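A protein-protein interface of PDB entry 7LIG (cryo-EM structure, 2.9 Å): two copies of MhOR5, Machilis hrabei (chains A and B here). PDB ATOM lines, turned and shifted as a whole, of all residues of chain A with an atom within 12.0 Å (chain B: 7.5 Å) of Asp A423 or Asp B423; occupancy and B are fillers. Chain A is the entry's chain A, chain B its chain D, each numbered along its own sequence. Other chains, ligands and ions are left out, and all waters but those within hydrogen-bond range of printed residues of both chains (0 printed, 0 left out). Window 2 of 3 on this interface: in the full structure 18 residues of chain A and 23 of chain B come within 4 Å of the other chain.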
ATOM      1  N   LEU A 249       4.127  17.722  26.218  1.00  0.00           N
ATOM      2  CA  LEU A 249       4.609  16.589  26.995  1.00  0.00           C
ATOM      3  C   LEU A 249       4.399  16.784  28.489  1.00  0.00           C
ATOM      4  O   LEU A 249       4.345  15.801  29.235  1.00  0.00           O
ATOM      5  CB  LEU A 249       6.086  16.331  26.703  1.00  0.00           C
ATOM      6  CG  LEU A 249       6.512  14.877  26.884  1.00  0.00           C
ATOM      7  CD1 LEU A 249       5.528  13.955  26.206  1.00  0.00           C
ATOM      8  CD2 LEU A 249       7.888  14.672  26.315  1.00  0.00           C
ATOM      9  N   ASP A 321      -4.577  14.651  22.843  1.00  0.00           N
ATOM     10  CA  ASP A 321      -3.698  13.488  22.878  1.00  0.00           C
ATOM     11  C   ASP A 321      -2.892  13.337  21.583  1.00  0.00           C
ATOM     12  O   ASP A 321      -1.732  13.739  21.524  1.00  0.00           O
ATOM     13  CB  ASP A 321      -4.512  12.220  23.173  1.00  0.00           C
ATOM     14  CG  ASP A 321      -5.866  12.215  22.484  1.00  0.00           C
ATOM     15  OD1 ASP A 321      -6.207  13.223  21.833  1.00  0.00           O
ATOM     16  OD2 ASP A 321      -6.584  11.199  22.592  1.00  0.00           O
ATOM     17  N   ALA A 322      -3.502  12.760  20.546  1.00  0.00           N
ATOM     18  CA  ALA A 322      -2.783  12.540  19.296  1.00  0.00           C
ATOM     19  C   ALA A 322      -2.750  13.798  18.441  1.00  0.00           C
ATOM     20  O   ALA A 322      -1.752  14.064  17.757  1.00  0.00           O
ATOM     21  CB  ALA A 322      -3.418  11.387  18.521  1.00  0.00           C
ATOM     22  N   LEU A 325       0.110  16.142  18.683  1.00  0.00           N
ATOM     23  CA  LEU A 325       1.314  15.621  18.045  1.00  0.00           C
ATOM     24  C   LEU A 325       1.236  15.740  16.530  1.00  0.00           C
ATOM     25  O   LEU A 325       2.247  16.023  15.874  1.00  0.00           O
ATOM     26  CB  LEU A 325       1.538  14.172  18.461  1.00  0.00           C
ATOM     27  CG  LEU A 325       2.193  14.000  19.827  1.00  0.00           C
ATOM     28  CD1 LEU A 325       2.304  12.534  20.171  1.00  0.00           C
ATOM     29  CD2 LEU A 325       3.556  14.661  19.848  1.00  0.00           C
ATOM     30  N   LYS A 417       9.473  12.544  31.942  1.00  0.00           N
ATOM     31  CA  LYS A 417       8.104  12.213  31.565  1.00  0.00           C
ATOM     32  C   LYS A 417       8.073  11.292  30.353  1.00  0.00           C
ATOM     33  O   LYS A 417       7.166  10.461  30.219  1.00  0.00           O
ATOM     34  CB  LYS A 417       7.317  13.491  31.291  1.00  0.00           C
ATOM     35  CG  LYS A 417       7.649  14.628  32.240  1.00  0.00           C
ATOM     36  CD  LYS A 417       7.146  14.340  33.643  1.00  0.00           C
ATOM     37  CE  LYS A 417       5.673  14.674  33.782  1.00  0.00           C
ATOM     38  NZ  LYS A 417       5.430  16.137  33.674  1.00  0.00           N
ATOM     39  N   LEU A 418       9.077  11.409  29.479  1.00  0.00           N
ATOM     40  CA  LEU A 418       9.143  10.591  28.270  1.00  0.00           C
ATOM     41  C   LEU A 418       9.305   9.115  28.601  1.00  0.00           C
ATOM     42  O   LEU A 418       8.856   8.247  27.846  1.00  0.00           O
ATOM     43  CB  LEU A 418      10.298  11.070  27.395  1.00  0.00           C
ATOM     44  CG  LEU A 418      10.507  10.410  26.038  1.00  0.00           C
ATOM     45  CD1 LEU A 418       9.569  11.020  25.032  1.00  0.00           C
ATOM     46  CD2 LEU A 418      11.944  10.570  25.599  1.00  0.00           C
ATOM     47  N   VAL A 419       9.925   8.811  29.737  1.00  0.00           N
ATOM     48  CA  VAL A 419      10.114   7.438  30.179  1.00  0.00           C
ATOM     49  C   VAL A 419       8.768   6.879  30.627  1.00  0.00           C
ATOM     50  O   VAL A 419       8.491   5.684  30.464  1.00  0.00           O
ATOM     51  CB  VAL A 419      11.171   7.384  31.298  1.00  0.00           C
ATOM     52  CG1 VAL A 419      11.323   5.986  31.870  1.00  0.00           C
ATOM     53  CG2 VAL A 419      12.497   7.883  30.771  1.00  0.00           C
ATOM     54  N   LEU A 420       7.887   7.749  31.127  1.00  0.00           N
ATOM     55  CA  LEU A 420       6.619   7.291  31.681  1.00  0.00           C
ATOM     56  C   LEU A 420       5.465   7.435  30.698  1.00  0.00           C
ATOM     57  O   LEU A 420       4.308   7.234  31.079  1.00  0.00           O
ATOM     58  CB  LEU A 420       6.297   8.035  32.976  1.00  0.00           C
ATOM     59  CG  LEU A 420       7.364   7.918  34.058  1.00  0.00           C
ATOM     60  CD1 LEU A 420       6.900   8.604  35.325  1.00  0.00           C
ATOM     61  CD2 LEU A 420       7.687   6.462  34.322  1.00  0.00           C
ATOM     62  N   ALA A 421       5.744   7.775  29.448  1.00  0.00           N
ATOM     63  CA  ALA A 421       4.692   7.892  28.455  1.00  0.00           C
ATOM     64  C   ALA A 421       4.418   6.542  27.806  1.00  0.00           C
ATOM     65  O   ALA A 421       5.091   5.546  28.074  1.00  0.00           O
ATOM     66  CB  ALA A 421       5.066   8.920  27.391  1.00  0.00           C
ATOM     67  N   SER A 422       3.421   6.524  26.925  1.00  0.00           N
ATOM     68  CA  SER A 422       3.035   5.297  26.247  1.00  0.00           C
ATOM     69  C   SER A 422       4.025   4.964  25.132  1.00  0.00           C
ATOM     70  O   SER A 422       5.071   5.595  24.972  1.00  0.00           O
ATOM     71  CB  SER A 422       1.626   5.422  25.672  1.00  0.00           C
ATOM     72  OG  SER A 422       1.592   6.366  24.618  1.00  0.00           O
ATOM     73  N   ASP A 423       3.681   3.938  24.354  1.00  0.00           N
ATOM     74  CA  ASP A 423       4.511   3.592  23.207  1.00  0.00           C
ATOM     75  C   ASP A 423       4.338   4.593  22.078  1.00  0.00           C
ATOM     76  O   ASP A 423       5.270   4.819  21.294  1.00  0.00           O
ATOM     77  CB  ASP A 423       4.172   2.187  22.721  1.00  0.00           C
ATOM     78  CG  ASP A 423       5.351   1.503  22.068  1.00  0.00           C
ATOM     79  OD1 ASP A 423       5.143   0.476  21.389  1.00  0.00           O
ATOM     80  OD2 ASP A 423       6.487   1.988  22.242  1.00  0.00           O
ATOM     81  N   HIS A 424       3.157   5.208  21.993  1.00  0.00           N
ATOM     82  CA  HIS A 424       2.862   6.153  20.922  1.00  0.00           C
ATOM     83  C   HIS A 424       3.735   7.395  21.027  1.00  0.00           C
ATOM     84  O   HIS A 424       4.325   7.841  20.034  1.00  0.00           O
ATOM     85  CB  HIS A 424       1.384   6.532  20.974  1.00  0.00           C
ATOM     86  CG  HIS A 424       0.828   6.983  19.661  1.00  0.00           C
ATOM     87  ND1 HIS A 424      -0.282   6.405  19.087  1.00  0.00           N
ATOM     88  CD2 HIS A 424       1.227   7.959  18.814  1.00  0.00           C
ATOM     89  CE1 HIS A 424      -0.542   7.003  17.939  1.00  0.00           C
ATOM     90  NE2 HIS A 424       0.359   7.951  17.750  1.00  0.00           N
ATOM     91  N   VAL A 425       3.838   7.959  22.229  1.00  0.00           N
ATOM     92  CA  VAL A 425       4.651   9.153  22.421  1.00  0.00           C
ATOM     93  C   VAL A 425       6.127   8.823  22.259  1.00  0.00           C
ATOM     94  O   VAL A 425       6.876   9.566  21.618  1.00  0.00           O
ATOM     95  CB  VAL A 425       4.355   9.783  23.790  1.00  0.00           C
ATOM     96  CG1 VAL A 425       5.119  11.068  23.943  1.00  0.00           C
ATOM     97  CG2 VAL A 425       2.869  10.032  23.940  1.00  0.00           C
ATOM     98  N   ARG A 426       6.562   7.687  22.805  1.00  0.00           N
ATOM     99  CA  ARG A 426       7.957   7.284  22.671  1.00  0.00           C
ATOM    100  C   ARG A 426       8.335   6.898  21.249  1.00  0.00           C
ATOM    101  O   ARG A 426       9.530   6.816  20.951  1.00  0.00           O
ATOM    102  CB  ARG A 426       8.271   6.126  23.617  1.00  0.00           C
ATOM    103  CG  ARG A 426       8.714   6.569  24.993  1.00  0.00           C
ATOM    104  CD  ARG A 426       9.011   5.388  25.890  1.00  0.00           C
ATOM    105  NE  ARG A 426       7.786   4.763  26.367  1.00  0.00           N
ATOM    106  CZ  ARG A 426       7.396   3.543  26.026  1.00  0.00           C
ATOM    107  NH1 ARG A 426       6.264   3.049  26.505  1.00  0.00           N
ATOM    108  NH2 ARG A 426       8.140   2.814  25.209  1.00  0.00           N
ATOM    109  N   SER A 427       7.366   6.659  20.371  1.00  0.00           N
ATOM    110  CA  SER A 427       7.662   6.482  18.957  1.00  0.00           C
ATOM    111  C   SER A 427       7.645   7.790  18.179  1.00  0.00           C
ATOM    112  O   SER A 427       8.536   8.026  17.354  1.00  0.00           O
ATOM    113  CB  SER A 427       6.667   5.507  18.328  1.00  0.00           C
ATOM    114  OG  SER A 427       6.905   5.376  16.941  1.00  0.00           O
ATOM    115  N   THR A 428       6.667   8.662  18.432  1.00  0.00           N
ATOM    116  CA  THR A 428       6.590   9.899  17.662  1.00  0.00           C
ATOM    117  C   THR A 428       7.684  10.882  18.059  1.00  0.00           C
ATOM    118  O   THR A 428       8.200  11.609  17.205  1.00  0.00           O
ATOM    119  CB  THR A 428       5.218  10.544  17.811  1.00  0.00           C
ATOM    120  OG1 THR A 428       4.994  10.875  19.184  1.00  0.00           O
ATOM    121  CG2 THR A 428       4.137   9.614  17.313  1.00  0.00           C
ATOM    122  N   ILE A 429       8.059  10.920  19.341  1.00  0.00           N
ATOM    123  CA  ILE A 429       9.163  11.782  19.757  1.00  0.00           C
ATOM    124  C   ILE A 429      10.473  11.279  19.166  1.00  0.00           C
ATOM    125  O   ILE A 429      11.332  12.070  18.751  1.00  0.00           O
ATOM    126  CB  ILE A 429       9.214  11.875  21.293  1.00  0.00           C
ATOM    127  CG1 ILE A 429       7.982  12.606  21.818  1.00  0.00           C
ATOM    128  CG2 ILE A 429      10.438  12.624  21.760  1.00  0.00           C
ATOM    129  CD1 ILE A 429       7.782  13.962  21.215  1.00  0.00           C
ATOM    130  N   GLN A 430      10.620   9.956  19.061  1.00  0.00           N
ATOM    131  CA  GLN A 430      11.788   9.381  18.405  1.00  0.00           C
ATOM    132  C   GLN A 430      11.832   9.751  16.929  1.00  0.00           C
ATOM    133  O   GLN A 430      12.900  10.082  16.399  1.00  0.00           O
ATOM    134  CB  GLN A 430      11.781   7.865  18.573  1.00  0.00           C
ATOM    135  CG  GLN A 430      12.939   7.169  17.907  1.00  0.00           C
ATOM    136  CD  GLN A 430      14.260   7.648  18.442  1.00  0.00           C
ATOM    137  OE1 GLN A 430      14.452   7.735  19.651  1.00  0.00           O
ATOM    138  NE2 GLN A 430      15.185   7.962  17.546  1.00  0.00           N
ATOM    139  N   ALA A 431      10.674   9.736  16.263  1.00  0.00           N
ATOM    140  CA  ALA A 431      10.619  10.114  14.853  1.00  0.00           C
ATOM    141  C   ALA A 431      10.947  11.591  14.661  1.00  0.00           C
ATOM    142  O   ALA A 431      11.691  11.959  13.741  1.00  0.00           O
ATOM    143  CB  ALA A 431       9.242   9.789  14.280  1.00  0.00           C
ATOM    144  N   ILE A 432      10.415  12.448  15.538  1.00  0.00           N
ATOM    145  CA  ILE A 432      10.696  13.880  15.474  1.00  0.00           C
ATOM    146  C   ILE A 432      12.181  14.143  15.691  1.00  0.00           C
ATOM    147  O   ILE A 432      12.787  14.959  14.989  1.00  0.00           O
ATOM    148  CB  ILE A 432       9.826  14.637  16.495  1.00  0.00           C
ATOM    149  CG1 ILE A 432       8.369  14.655  16.042  1.00  0.00           C
ATOM    150  CG2 ILE A 432      10.294  16.062  16.676  1.00  0.00           C
ATOM    151  CD1 ILE A 432       7.442  15.306  17.033  1.00  0.00           C
ATOM    152  N   ARG A 435      14.289  12.962  12.665  1.00  0.00           N
ATOM    153  CA  ARG A 435      14.157  13.888  11.546  1.00  0.00           C
ATOM    154  C   ARG A 435      14.840  15.215  11.848  1.00  0.00           C
ATOM    155  O   ARG A 435      15.360  15.872  10.941  1.00  0.00           O
ATOM    156  CB  ARG A 435      12.689  14.114  11.202  1.00  0.00           C
ATOM    157  CG  ARG A 435      12.213  13.297  10.024  1.00  0.00           C
ATOM    158  CD  ARG A 435      11.768  11.929  10.478  1.00  0.00           C
ATOM    159  NE  ARG A 435      11.595  11.002   9.372  1.00  0.00           N
ATOM    160  CZ  ARG A 435      11.235   9.736   9.524  1.00  0.00           C
ATOM    161  NH1 ARG A 435      11.010   9.257  10.738  1.00  0.00           N
ATOM    162  NH2 ARG A 435      11.096   8.952   8.467  1.00  0.00           N
ATOM    163  N   LEU B 420      -0.591   8.649  12.946  1.00  0.00           N
ATOM    164  CA  LEU B 420      -1.825   7.884  13.086  1.00  0.00           C
ATOM    165  C   LEU B 420      -1.713   6.482  12.500  1.00  0.00           C
ATOM    166  O   LEU B 420      -2.721   5.777  12.406  1.00  0.00           O
ATOM    167  CB  LEU B 420      -2.994   8.627  12.442  1.00  0.00           C
ATOM    168  CG  LEU B 420      -3.234  10.029  12.988  1.00  0.00           C
ATOM    169  CD1 LEU B 420      -4.470  10.630  12.356  1.00  0.00           C
ATOM    170  CD2 LEU B 420      -3.367   9.989  14.497  1.00  0.00           C
ATOM    171  N   ALA B 421      -0.520   6.060  12.107  1.00  0.00           N
ATOM    172  CA  ALA B 421      -0.342   4.720  11.575  1.00  0.00           C
ATOM    173  C   ALA B 421      -0.091   3.728  12.703  1.00  0.00           C
ATOM    174  O   ALA B 421       0.017   4.092  13.874  1.00  0.00           O
ATOM    175  CB  ALA B 421       0.812   4.685  10.578  1.00  0.00           C
ATOM    176  N   SER B 422       0.021   2.456  12.329  1.00  0.00           N
ATOM    177  CA  SER B 422       0.238   1.400  13.304  1.00  0.00           C
ATOM    178  C   SER B 422       1.692   1.387  13.770  1.00  0.00           C
ATOM    179  O   SER B 422       2.491   2.269  13.450  1.00  0.00           O
ATOM    180  CB  SER B 422      -0.131   0.040  12.713  1.00  0.00           C
ATOM    181  OG  SER B 422       0.766  -0.321  11.679  1.00  0.00           O
ATOM    182  N   ASP B 423       2.031   0.364  14.553  1.00  0.00           N
ATOM    183  CA  ASP B 423       3.414   0.210  14.982  1.00  0.00           C
ATOM    184  C   ASP B 423       4.293  -0.283  13.845  1.00  0.00           C
ATOM    185  O   ASP B 423       5.492   0.024  13.803  1.00  0.00           O
ATOM    186  CB  ASP B 423       3.493  -0.753  16.162  1.00  0.00           C
ATOM    187  CG  ASP B 423       4.662  -0.456  17.072  1.00  0.00           C
ATOM    188  OD1 ASP B 423       5.001  -1.319  17.906  1.00  0.00           O
ATOM    189  OD2 ASP B 423       5.236   0.646  16.957  1.00  0.00           O
ATOM    190  N   HIS B 424       3.706  -1.037  12.913  1.00  0.00           N
ATOM    191  CA  HIS B 424       4.461  -1.603  11.801  1.00  0.00           C
ATOM    192  C   HIS B 424       4.995  -0.513  10.884  1.00  0.00           C
ATOM    193  O   HIS B 424       6.174  -0.519  10.509  1.00  0.00           O
ATOM    194  CB  HIS B 424       3.572  -2.570  11.025  1.00  0.00           C
ATOM    195  CG  HIS B 424       4.326  -3.622  10.280  1.00  0.00           C
ATOM    196  ND1 HIS B 424       4.080  -4.968  10.442  1.00  0.00           N
ATOM    197  CD2 HIS B 424       5.318  -3.528   9.364  1.00  0.00           C
ATOM    198  CE1 HIS B 424       4.891  -5.658   9.662  1.00  0.00           C
ATOM    199  NE2 HIS B 424       5.652  -4.809   8.996  1.00  0.00           N
ATOM    200  N   VAL B 425       4.137   0.442  10.520  1.00  0.00           N
ATOM    201  CA  VAL B 425       4.561   1.522   9.640  1.00  0.00           C
ATOM    202  C   VAL B 425       5.542   2.438  10.358  1.00  0.00           C
ATOM    203  O   VAL B 425       6.558   2.847   9.789  1.00  0.00           O
ATOM    204  CB  VAL B 425       3.338   2.294   9.122  1.00  0.00           C
ATOM    205  CG1 VAL B 425       3.770   3.344   8.138  1.00  0.00           C
ATOM    206  CG2 VAL B 425       2.353   1.341   8.478  1.00  0.00           C
ATOM    207  N   ARG B 426       5.276   2.744  11.628  1.00  0.00           N
ATOM    208  CA  ARG B 426       6.180   3.592  12.394  1.00  0.00           C
ATOM    209  C   ARG B 426       7.512   2.926  12.699  1.00  0.00           C
ATOM    210  O   ARG B 426       8.456   3.624  13.083  1.00  0.00           O
ATOM    211  CB  ARG B 426       5.521   4.036  13.698  1.00  0.00           C
ATOM    212  CG  ARG B 426       4.716   5.311  13.569  1.00  0.00           C
ATOM    213  CD  ARG B 426       4.084   5.707  14.884  1.00  0.00           C
ATOM    214  NE  ARG B 426       2.925   4.879  15.185  1.00  0.00           N
ATOM    215  CZ  ARG B 426       2.869   4.019  16.193  1.00  0.00           C
ATOM    216  NH1 ARG B 426       1.775   3.302  16.395  1.00  0.00           N
ATOM    217  NH2 ARG B 426       3.910   3.879  16.999  1.00  0.00           N
ATOM    218  N   SER B 427       7.621   1.609  12.543  1.00  0.00           N
ATOM    219  CA  SER B 427       8.914   0.947  12.627  1.00  0.00           C
ATOM    220  C   SER B 427       9.629   0.870  11.286  1.00  0.00           C
ATOM    221  O   SER B 427      10.838   1.126  11.216  1.00  0.00           O
ATOM    222  CB  SER B 427       8.749  -0.463  13.193  1.00  0.00           C
ATOM    223  OG  SER B 427       9.991  -1.138  13.219  1.00  0.00           O
ATOM    224  N   THR B 428       8.913   0.546  10.206  1.00  0.00           N
ATOM    225  CA  THR B 428       9.580   0.408   8.916  1.00  0.00           C
ATOM    226  C   THR B 428       9.990   1.758   8.342  1.00  0.00           C
ATOM    227  O   THR B 428      11.036   1.862   7.696  1.00  0.00           O
ATOM    228  CB  THR B 428       8.694  -0.343   7.929  1.00  0.00           C
ATOM    229  OG1 THR B 428       7.489   0.395   7.715  1.00  0.00           O
ATOM    230  CG2 THR B 428       8.378  -1.727   8.442  1.00  0.00           C
ATOM    231  N   ILE B 429       9.190   2.804   8.567  1.00  0.00           N
ATOM    232  CA  ILE B 429       9.580   4.137   8.113  1.00  0.00           C
ATOM    233  C   ILE B 429      10.793   4.624   8.897  1.00  0.00           C
ATOM    234  O   ILE B 429      11.697   5.262   8.340  1.00  0.00           O
ATOM    235  CB  ILE B 429       8.389   5.106   8.225  1.00  0.00           C
ATOM    236  CG1 ILE B 429       7.293   4.709   7.240  1.00  0.00           C
ATOM    237  CG2 ILE B 429       8.802   6.526   7.919  1.00  0.00           C
ATOM    238  CD1 ILE B 429       7.763   4.612   5.821  1.00  0.00           C
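The side-chain hydroxyl (OG) of Ser A427 lies within hydrogen-bond range of the guanidinium group (NH2) of Arg B426.
The guanidinium group of Arg A426 is in salt-bridge range of the side-chain carboxylate of Asp A423, 3.5 Å away.
The backbone carbonyl oxygen (O) of Ala B421 lies within hydrogen-bond range of the guanidinium group (NH1) of Arg B426 (3.2 Å).
NE of Arg B426 lies within hydrogen-bond range of O of Ser B422 (3.2 Å).
NH2 of Arg B426 is in salt-bridge range of OD2 of Asp B423, at 3.5 Å.
Asp A423 touches Asp B423.
Ile B429 touches Arg A435.
Asp A423 touches just one residue of chain B: Asp B423 (3.9 Å).
Printed residues of chain B within 4 Å of Ser A427: Arg B426.
Of the printed residues of chain B, Arg A435 touches Ile B429.
Leu B420 touches none of the printed residues of chain A.
Ala B421 touches none of the printed residues of chain A.
Asp B423 touches just one residue of chain A: Asp A423 (3.9 Å).
Arg B426 touches just one residue of chain A: Ser A427 (3.3 Å).
No residue of chain A comes within 4 Å of Ser B427.
Of the printed residues of chain A, Ile B429 touches Arg A435 (3.4 Å).
Of the 21 printed residues of chain A, 3 touch a printed residue of chain B.
Hydrophobic or aromatic side chains of chain B that line the printed part of chain A: Ile B429.
Among the printed residues, 3 pairs touch across the chains.
Among the printed residues, no Asp or Glu carboxylate lies within 4 Å of a Lys or Arg side-chain nitrogen of the other chain.
Asp B423 touches its own counterpart, Asp A423.
Ser A427 touches Arg B426, but with the chains exchanged Arg A426 does not touch Ser B427 (10.1 Å).
Of the 3 pairs that touch across the chains among the printed residues, 1 has its exchanged pair printed and touching as well.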
